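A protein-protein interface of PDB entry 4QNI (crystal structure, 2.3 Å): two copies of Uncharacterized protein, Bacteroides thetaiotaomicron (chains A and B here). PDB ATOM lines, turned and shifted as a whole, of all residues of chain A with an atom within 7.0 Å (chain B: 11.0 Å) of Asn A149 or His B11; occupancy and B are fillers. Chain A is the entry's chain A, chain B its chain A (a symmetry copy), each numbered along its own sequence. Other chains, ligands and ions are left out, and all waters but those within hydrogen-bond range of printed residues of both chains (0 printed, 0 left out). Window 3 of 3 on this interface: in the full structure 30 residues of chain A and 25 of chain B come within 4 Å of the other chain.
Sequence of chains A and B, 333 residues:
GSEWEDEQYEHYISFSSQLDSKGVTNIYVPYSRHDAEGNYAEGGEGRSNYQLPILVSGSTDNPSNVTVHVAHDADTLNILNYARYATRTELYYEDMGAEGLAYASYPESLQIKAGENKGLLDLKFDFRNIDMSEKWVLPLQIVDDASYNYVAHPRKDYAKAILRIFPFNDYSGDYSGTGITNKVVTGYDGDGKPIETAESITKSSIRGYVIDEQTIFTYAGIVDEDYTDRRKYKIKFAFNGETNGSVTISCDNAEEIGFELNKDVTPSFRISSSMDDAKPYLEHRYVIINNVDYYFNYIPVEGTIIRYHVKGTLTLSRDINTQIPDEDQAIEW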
ATOM      1  N   VAL A  56      -0.228  -1.752  -5.140  1.00  0.00           N
ATOM      2  CA  VAL A  56      -1.334  -2.698  -5.329  1.00  0.00           C
ATOM      3  C   VAL A  56      -1.278  -3.799  -4.282  1.00  0.00           C
ATOM      4  O   VAL A  56      -0.258  -4.464  -4.147  1.00  0.00           O
ATOM      5  CB  VAL A  56      -1.315  -3.332  -6.750  1.00  0.00           C
ATOM      6  CG1 VAL A  56      -2.613  -4.085  -7.031  1.00  0.00           C
ATOM      7  CG2 VAL A  56      -1.046  -2.295  -7.839  1.00  0.00           C
ATOM      8  N   SER A  57      -2.401  -4.035  -3.595  1.00  0.00           N
ATOM      9  CA  SER A  57      -2.580  -5.140  -2.639  1.00  0.00           C
ATOM     10  C   SER A  57      -3.084  -6.423  -3.390  1.00  0.00           C
ATOM     11  O   SER A  57      -3.488  -6.331  -4.543  1.00  0.00           O
ATOM     12  CB  SER A  57      -3.572  -4.726  -1.559  1.00  0.00           C
ATOM     13  OG  SER A  57      -4.859  -4.538  -2.129  1.00  0.00           O
ATOM     14  N   GLY A  58      -3.044  -7.584  -2.738  1.00  0.00           N
ATOM     15  CA  GLY A  58      -3.489  -8.862  -3.301  1.00  0.00           C
ATOM     16  C   GLY A  58      -2.715  -9.399  -4.498  1.00  0.00           C
ATOM     17  O   GLY A  58      -1.609  -8.951  -4.819  1.00  0.00           O
ATOM     18  N   PRO A  63      -3.801 -12.932  -7.678  1.00  0.00           N
ATOM     19  CA  PRO A  63      -2.606 -13.384  -8.410  1.00  0.00           C
ATOM     20  C   PRO A  63      -2.821 -13.337  -9.934  1.00  0.00           C
ATOM     21  O   PRO A  63      -2.368 -14.228 -10.665  1.00  0.00           O
ATOM     22  CB  PRO A  63      -2.365 -14.806  -7.875  1.00  0.00           C
ATOM     23  CG  PRO A  63      -3.588 -15.159  -7.071  1.00  0.00           C
ATOM     24  CD  PRO A  63      -4.173 -13.867  -6.602  1.00  0.00           C
ATOM     25  N   SER A  64      -3.500 -12.265 -10.408  1.00  0.00           N
ATOM     26  CA  SER A  64      -3.787 -11.972 -11.823  1.00  0.00           C
ATOM     27  C   SER A  64      -3.156 -10.615 -12.224  1.00  0.00           C
ATOM     28  O   SER A  64      -2.536  -9.967 -11.368  1.00  0.00           O
ATOM     29  CB  SER A  64      -5.296 -11.965 -12.071  1.00  0.00           C
ATOM     30  OG  SER A  64      -5.604 -11.797 -13.447  1.00  0.00           O
ATOM     31  N   ASN A  65      -3.302 -10.202 -13.518  1.00  0.00           N
ATOM     32  CA  ASN A  65      -2.785  -8.933 -14.067  1.00  0.00           C
ATOM     33  C   ASN A  65      -3.772  -7.792 -13.825  1.00  0.00           C
ATOM     34  O   ASN A  65      -4.970  -7.941 -14.095  1.00  0.00           O
ATOM     35  CB  ASN A  65      -2.487  -9.057 -15.567  1.00  0.00           C
ATOM     36  CG  ASN A  65      -1.225  -9.809 -15.906  1.00  0.00           C
ATOM     37  OD1 ASN A  65      -0.250  -9.840 -15.143  1.00  0.00           O
ATOM     38  ND2 ASN A  65      -1.196 -10.392 -17.095  1.00  0.00           N
ATOM     39  N   VAL A  66      -3.271  -6.650 -13.324  1.00  0.00           N
ATOM     40  CA  VAL A  66      -4.117  -5.495 -12.997  1.00  0.00           C
ATOM     41  C   VAL A  66      -3.792  -4.320 -13.923  1.00  0.00           C
ATOM     42  O   VAL A  66      -2.627  -3.956 -14.078  1.00  0.00           O
ATOM     43  CB  VAL A  66      -3.984  -5.104 -11.491  1.00  0.00           C
ATOM     44  CG1 VAL A  66      -4.805  -3.862 -11.146  1.00  0.00           C
ATOM     45  CG2 VAL A  66      -4.377  -6.266 -10.579  1.00  0.00           C
ATOM     46  N   THR A  67      -4.825  -3.740 -14.535  1.00  0.00           N
ATOM     47  CA  THR A  67      -4.712  -2.553 -15.369  1.00  0.00           C
ATOM     48  C   THR A  67      -5.277  -1.417 -14.547  1.00  0.00           C
ATOM     49  O   THR A  67      -6.470  -1.407 -14.248  1.00  0.00           O
ATOM     50  CB  THR A  67      -5.413  -2.739 -16.722  1.00  0.00           C
ATOM     51  OG1 THR A  67      -4.807  -3.828 -17.410  1.00  0.00           O
ATOM     52  CG2 THR A  67      -5.358  -1.483 -17.592  1.00  0.00           C
ATOM     53  N   ALA A 114       1.406  -9.766 -12.759  1.00  0.00           N
ATOM     54  CA  ALA A 114       0.678 -10.740 -11.942  1.00  0.00           C
ATOM     55  C   ALA A 114       1.024 -10.743 -10.429  1.00  0.00           C
ATOM     56  O   ALA A 114       0.129 -10.504  -9.610  1.00  0.00           O
ATOM     57  CB  ALA A 114       0.865 -12.138 -12.513  1.00  0.00           C
ATOM     58  N   GLU A 116       3.289  -8.756  -8.818  1.00  0.00           N
ATOM     59  CA  GLU A 116       3.910  -7.511  -8.389  1.00  0.00           C
ATOM     60  C   GLU A 116       2.946  -6.695  -7.523  1.00  0.00           C
ATOM     61  O   GLU A 116       1.725  -6.757  -7.711  1.00  0.00           O
ATOM     62  CB  GLU A 116       4.403  -6.696  -9.594  1.00  0.00           C
ATOM     63  CG  GLU A 116       5.550  -7.335 -10.363  1.00  0.00           C
ATOM     64  CD  GLU A 116       6.773  -7.722  -9.551  1.00  0.00           C
ATOM     65  OE1 GLU A 116       7.485  -6.810  -9.072  1.00  0.00           O
ATOM     66  OE2 GLU A 116       7.024  -8.941  -9.405  1.00  0.00           O
ATOM     67  N   ASP A 144     -11.999   4.704 -10.436  1.00  0.00           N
ATOM     68  CA  ASP A 144     -12.766   3.555  -9.969  1.00  0.00           C
ATOM     69  C   ASP A 144     -13.900   3.228 -10.944  1.00  0.00           C
ATOM     70  O   ASP A 144     -14.558   4.147 -11.455  1.00  0.00           O
ATOM     71  CB  ASP A 144     -13.316   3.814  -8.551  1.00  0.00           C
ATOM     72  CG  ASP A 144     -12.891   2.776  -7.528  1.00  0.00           C
ATOM     73  OD1 ASP A 144     -12.550   1.634  -7.938  1.00  0.00           O
ATOM     74  OD2 ASP A 144     -12.946   3.082  -6.318  1.00  0.00           O
ATOM     75  N   ASP A 145     -14.109   1.922 -11.228  1.00  0.00           N
ATOM     76  CA  ASP A 145     -15.190   1.448 -12.105  1.00  0.00           C
ATOM     77  C   ASP A 145     -15.521  -0.016 -11.831  1.00  0.00           C
ATOM     78  O   ASP A 145     -14.647  -0.780 -11.413  1.00  0.00           O
ATOM     79  CB  ASP A 145     -14.857   1.644 -13.596  1.00  0.00           C
ATOM     80  CG  ASP A 145     -16.057   1.852 -14.500  1.00  0.00           C
ATOM     81  OD1 ASP A 145     -16.914   2.706 -14.168  1.00  0.00           O
ATOM     82  OD2 ASP A 145     -16.102   1.219 -15.574  1.00  0.00           O
ATOM     83  N   ALA A 146     -16.800  -0.395 -12.074  1.00  0.00           N
ATOM     84  CA  ALA A 146     -17.329  -1.752 -11.893  1.00  0.00           C
ATOM     85  C   ALA A 146     -16.671  -2.755 -12.865  1.00  0.00           C
ATOM     86  O   ALA A 146     -16.498  -3.925 -12.505  1.00  0.00           O
ATOM     87  CB  ALA A 146     -18.832  -1.746 -12.089  1.00  0.00           C
ATOM     88  N   SER A 147     -16.288  -2.276 -14.076  1.00  0.00           N
ATOM     89  CA  SER A 147     -15.602  -3.041 -15.131  1.00  0.00           C
ATOM     90  C   SER A 147     -14.218  -3.525 -14.678  1.00  0.00           C
ATOM     91  O   SER A 147     -13.835  -4.667 -14.964  1.00  0.00           O
ATOM     92  CB  SER A 147     -15.424  -2.193 -16.390  1.00  0.00           C
ATOM     93  OG  SER A 147     -16.319  -1.097 -16.457  1.00  0.00           O
ATOM     94  N   TYR A 148     -13.476  -2.631 -13.973  1.00  0.00           N
ATOM     95  CA  TYR A 148     -12.109  -2.817 -13.473  1.00  0.00           C
ATOM     96  C   TYR A 148     -11.999  -3.952 -12.431  1.00  0.00           C
ATOM     97  O   TYR A 148     -12.894  -4.144 -11.597  1.00  0.00           O
ATOM     98  CB  TYR A 148     -11.566  -1.500 -12.867  1.00  0.00           C
ATOM     99  CG  TYR A 148     -11.615  -0.272 -13.762  1.00  0.00           C
ATOM    100  CD1 TYR A 148     -11.777  -0.391 -15.142  1.00  0.00           C
ATOM    101  CD2 TYR A 148     -11.435   1.004 -13.238  1.00  0.00           C
ATOM    102  CE1 TYR A 148     -11.845   0.736 -15.964  1.00  0.00           C
ATOM    103  CE2 TYR A 148     -11.461   2.137 -14.056  1.00  0.00           C
ATOM    104  CZ  TYR A 148     -11.681   1.998 -15.417  1.00  0.00           C
ATOM    105  OH  TYR A 148     -11.718   3.106 -16.229  1.00  0.00           O
ATOM    106  N   ASN A 149     -10.867  -4.688 -12.492  1.00  0.00           N
ATOM    107  CA  ASN A 149     -10.516  -5.797 -11.592  1.00  0.00           C
ATOM    108  C   ASN A 149      -9.719  -5.253 -10.379  1.00  0.00           C
ATOM    109  O   ASN A 149      -8.715  -5.848  -9.974  1.00  0.00           O
ATOM    110  CB  ASN A 149      -9.719  -6.877 -12.352  1.00  0.00           C
ATOM    111  N   TYR A 150     -10.188  -4.110  -9.814  1.00  0.00           N
ATOM    112  CA  TYR A 150      -9.597  -3.403  -8.675  1.00  0.00           C
ATOM    113  C   TYR A 150     -10.543  -2.335  -8.106  1.00  0.00           C
ATOM    114  O   TYR A 150     -11.567  -1.999  -8.719  1.00  0.00           O
ATOM    115  CB  TYR A 150      -8.262  -2.752  -9.084  1.00  0.00           C
ATOM    116  CG  TYR A 150      -8.377  -1.495  -9.928  1.00  0.00           C
ATOM    117  CD1 TYR A 150      -8.549  -0.244  -9.335  1.00  0.00           C
ATOM    118  CD2 TYR A 150      -8.236  -1.544 -11.311  1.00  0.00           C
ATOM    119  CE1 TYR A 150      -8.579   0.921 -10.094  1.00  0.00           C
ATOM    120  CE2 TYR A 150      -8.266  -0.384 -12.081  1.00  0.00           C
ATOM    121  CZ  TYR A 150      -8.428   0.848 -11.466  1.00  0.00           C
ATOM    122  OH  TYR A 150      -8.465   2.004 -12.207  1.00  0.00           O
ATOM    123  N   VAL A 151     -10.157  -1.766  -6.944  1.00  0.00           N
ATOM    124  CA  VAL A 151     -10.850  -0.671  -6.260  1.00  0.00           C
ATOM    125  C   VAL A 151      -9.800   0.339  -5.764  1.00  0.00           C
ATOM    126  O   VAL A 151      -8.793  -0.061  -5.174  1.00  0.00           O
ATOM    127  CB  VAL A 151     -11.774  -1.166  -5.112  1.00  0.00           C
ATOM    128  CG1 VAL A 151     -12.208  -0.027  -4.196  1.00  0.00           C
ATOM    129  CG2 VAL A 151     -12.999  -1.888  -5.664  1.00  0.00           C
ATOM    130  N   ALA A 152     -10.034   1.644  -6.024  1.00  0.00           N
ATOM    131  CA  ALA A 152      -9.200   2.726  -5.509  1.00  0.00           C
ATOM    132  C   ALA A 152      -9.341   2.718  -3.995  1.00  0.00           C
ATOM    133  O   ALA A 152     -10.453   2.542  -3.495  1.00  0.00           O
ATOM    134  CB  ALA A 152      -9.642   4.060  -6.090  1.00  0.00           C
ATOM    135  N   HIS A 153      -8.219   2.824  -3.268  1.00  0.00           N
ATOM    136  CA  HIS A 153      -8.174   2.778  -1.805  1.00  0.00           C
ATOM    137  C   HIS A 153      -9.322   3.553  -1.156  1.00  0.00           C
ATOM    138  O   HIS A 153      -9.535   4.715  -1.528  1.00  0.00           O
ATOM    139  CB  HIS A 153      -6.845   3.315  -1.272  1.00  0.00           C
ATOM    140  CG  HIS A 153      -6.511   2.784   0.085  1.00  0.00           C
ATOM    141  ND1 HIS A 153      -7.142   3.258   1.222  1.00  0.00           N
ATOM    142  CD2 HIS A 153      -5.637   1.815   0.438  1.00  0.00           C
ATOM    143  CE1 HIS A 153      -6.629   2.569   2.224  1.00  0.00           C
ATOM    144  NE2 HIS A 153      -5.714   1.694   1.803  1.00  0.00           N
ATOM    145  N   TYR B   9     -13.582  -5.906  -6.564  1.00  0.00           N
ATOM    146  CA  TYR B   9     -12.759  -5.707  -5.370  1.00  0.00           C
ATOM    147  C   TYR B   9     -11.432  -6.470  -5.524  1.00  0.00           C
ATOM    148  O   TYR B   9     -10.826  -6.382  -6.601  1.00  0.00           O
ATOM    149  CB  TYR B   9     -13.528  -6.137  -4.100  1.00  0.00           C
ATOM    150  N   GLU B  10     -10.971  -7.186  -4.441  1.00  0.00           N
ATOM    151  CA  GLU B  10      -9.759  -8.024  -4.326  1.00  0.00           C
ATOM    152  C   GLU B  10      -8.427  -7.216  -4.304  1.00  0.00           C
ATOM    153  O   GLU B  10      -7.484  -7.609  -3.605  1.00  0.00           O
ATOM    154  CB  GLU B  10      -9.702  -9.095  -5.437  1.00  0.00           C
ATOM    155  N   HIS B  11      -8.363  -6.104  -5.072  1.00  0.00           N
ATOM    156  CA  HIS B  11      -7.186  -5.243  -5.211  1.00  0.00           C
ATOM    157  C   HIS B  11      -7.449  -3.801  -4.814  1.00  0.00           C
ATOM    158  O   HIS B  11      -8.305  -3.139  -5.404  1.00  0.00           O
ATOM    159  CB  HIS B  11      -6.682  -5.258  -6.667  1.00  0.00           C
ATOM    160  CG  HIS B  11      -6.305  -6.615  -7.159  1.00  0.00           C
ATOM    161  ND1 HIS B  11      -5.129  -7.224  -6.765  1.00  0.00           N
ATOM    162  CD2 HIS B  11      -6.980  -7.453  -7.979  1.00  0.00           C
ATOM    163  CE1 HIS B  11      -5.118  -8.402  -7.363  1.00  0.00           C
ATOM    164  NE2 HIS B  11      -6.211  -8.586  -8.104  1.00  0.00           N
ATOM    165  N   TYR B  12      -6.672  -3.308  -3.845  1.00  0.00           N
ATOM    166  CA  TYR B  12      -6.669  -1.917  -3.407  1.00  0.00           C
ATOM    167  C   TYR B  12      -5.469  -1.217  -4.061  1.00  0.00           C
ATOM    168  O   TYR B  12      -4.348  -1.722  -4.013  1.00  0.00           O
ATOM    169  CB  TYR B  12      -6.601  -1.806  -1.877  1.00  0.00           C
ATOM    170  CG  TYR B  12      -7.901  -1.936  -1.112  1.00  0.00           C
ATOM    171  CD1 TYR B  12      -9.129  -1.949  -1.772  1.00  0.00           C
ATOM    172  CD2 TYR B  12      -7.908  -2.001   0.280  1.00  0.00           C
ATOM    173  CE1 TYR B  12     -10.331  -2.049  -1.067  1.00  0.00           C
ATOM    174  CE2 TYR B  12      -9.102  -2.087   0.997  1.00  0.00           C
ATOM    175  CZ  TYR B  12     -10.313  -2.116   0.320  1.00  0.00           C
ATOM    176  OH  TYR B  12     -11.490  -2.205   1.033  1.00  0.00           O
ATOM    177  N   ILE B  13      -5.729  -0.095  -4.725  1.00  0.00           N
ATOM    178  CA  ILE B  13      -4.732   0.700  -5.433  1.00  0.00           C
ATOM    179  C   ILE B  13      -4.545   2.031  -4.727  1.00  0.00           C
ATOM    180  O   ILE B  13      -5.527   2.688  -4.379  1.00  0.00           O
ATOM    181  CB  ILE B  13      -5.158   0.921  -6.906  1.00  0.00           C
ATOM    182  CG1 ILE B  13      -5.778  -0.335  -7.579  1.00  0.00           C
ATOM    183  CG2 ILE B  13      -4.039   1.542  -7.714  1.00  0.00           C
ATOM    184  CD1 ILE B  13      -4.846  -1.464  -8.004  1.00  0.00           C
ATOM    185  N   SER B  14      -3.297   2.449  -4.546  1.00  0.00           N
ATOM    186  CA  SER B  14      -2.990   3.741  -3.922  1.00  0.00           C
ATOM    187  C   SER B  14      -1.627   4.290  -4.382  1.00  0.00           C
ATOM    188  O   SER B  14      -0.746   3.518  -4.738  1.00  0.00           O
ATOM    189  CB  SER B  14      -3.008   3.618  -2.399  1.00  0.00           C
ATOM    190  OG  SER B  14      -1.829   2.994  -1.937  1.00  0.00           O
ATOM    191  N   ASP B  75       2.473  -9.928   0.555  1.00  0.00           N
ATOM    192  CA  ASP B  75       1.930  -8.713  -0.084  1.00  0.00           C
ATOM    193  C   ASP B  75       2.089  -7.492   0.768  1.00  0.00           C
ATOM    194  O   ASP B  75       2.666  -6.525   0.296  1.00  0.00           O
ATOM    195  CB  ASP B  75       0.443  -8.867  -0.453  1.00  0.00           C
ATOM    196  CG  ASP B  75       0.176  -9.693  -1.678  1.00  0.00           C
ATOM    197  OD1 ASP B  75       0.953  -9.578  -2.656  1.00  0.00           O
ATOM    198  OD2 ASP B  75      -0.842 -10.417  -1.687  1.00  0.00           O
ATOM    199  N   ILE B  79       4.500  -4.133   0.066  1.00  0.00           N
ATOM    200  CA  ILE B  79       4.016  -2.735   0.096  1.00  0.00           C
ATOM    201  C   ILE B  79       4.856  -1.944   1.107  1.00  0.00           C
ATOM    202  O   ILE B  79       5.401  -0.892   0.765  1.00  0.00           O
ATOM    203  CB  ILE B  79       2.499  -2.621   0.417  1.00  0.00           C
ATOM    204  CG1 ILE B  79       1.601  -3.517  -0.466  1.00  0.00           C
ATOM    205  CG2 ILE B  79       2.011  -1.164   0.498  1.00  0.00           C
ATOM    206  CD1 ILE B  79       1.571  -3.209  -1.859  1.00  0.00           C
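The backbone carbonyl oxygen of Ser A57 is in hydrogen-bond range of a ring nitrogen (ND1) of His B11 (2.9 Å). The backbone NH (N) of Tyr B12 is in hydrogen-bond range of the side-chain hydroxyl (OG) of Ser A57 (2.8 Å). The backbone NH (N) of Val A151 lies within hydrogen-bond range of the backbone carbonyl oxygen (O) of His B11. The backbone NH (N) of Ile B13 lies within hydrogen-bond range of the backbone carbonyl oxygen (O) of Val A151, at 3.1 Å. The backbone NH (N) of His A153 lies within hydrogen-bond range of the backbone carbonyl oxygen (O) of Ile B13, 2.9 Å away. The backbone carbonyl oxygen (O) of Gly A58 sits close to the side-chain carboxylate (OD1) of Asp B75 (3.4 Å).
The backbone NH (N) of Ala A152 lies within hydrogen-bond range of the side-chain carboxylate (OD1) of Asp A144.
Among the printed residues, merely in contact across the chains: Asn A149 with His B11 (3.1 Å), Val A56 with Ile B79 (3.2 Å), Tyr A150 with Ile B13 (3.3 Å), Val A151 with Tyr B12 (3.3 Å), Val A56 with Tyr B12 (3.4 Å), Tyr A150 with His B11 (3.5 Å), Val A56 with Ile B13 (3.6 Å), Tyr A150 with Tyr B9 (3.8 Å), Ala A152 with Ile B13 (3.8 Å), Val A151 with Tyr B9 (3.8 Å), Val A66 with His B11 (3.9 Å), Gly A58 with His B11 (3.9 Å) and Val A66 with Ile B13 (3.95 Å).
Printed residues of chain B within 4 Å of Val A56: Tyr B12, Ile B13 and Ile B79. Of chain B, only His B11 (2.9 Å) and Tyr B12 (2.8 Å) come within 4 Å of Ser A57. Gly A58 touches two residues of chain B. No residue of chain B comes within 4 Å of Ser A64. Printed residues of chain B within 4 Å of Val A66: His B11 (3.9 Å) and Ile B13 (3.95 Å). Ala A114 touches none of the printed residues of chain B. Of the printed residues of chain B, Asn A149 touches His B11. Of chain B, only Tyr B9 (3.8 Å), His B11 (2.8 Å), Tyr B12 (3.3 Å) and Ile B13 (3.1 Å) come within 4 Å of Val A151. Of the printed residues of chain B, His A153 touches Ile B13. His B11 touches just these residues of chain A: Ser A57 (2.9 Å), Gly A58 (3.9 Å), Val A66 (3.9 Å), Asn A149 (3.1 Å), Tyr A150 (3.5 Å) and Val A151 (2.8 Å). Printed residues of chain A within 4 Å of Asp B75: Gly A58 (3.4 Å). The nearest printed residue of chain B that does not touch Asn A149 is Tyr B9 (4.01 Å). The nearest printed residue of chain B that does not touch Val A66 is Tyr B12 (7.5 Å).
Of the 20 printed residues of chain A, 9 touch a printed residue of chain B. Hydrophobic or aromatic side chains of chain A within 4 Å of the printed part of chain B: Val A56, Val A66, Tyr A150, Val A151 and His A153.
No position is printed for both chains.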
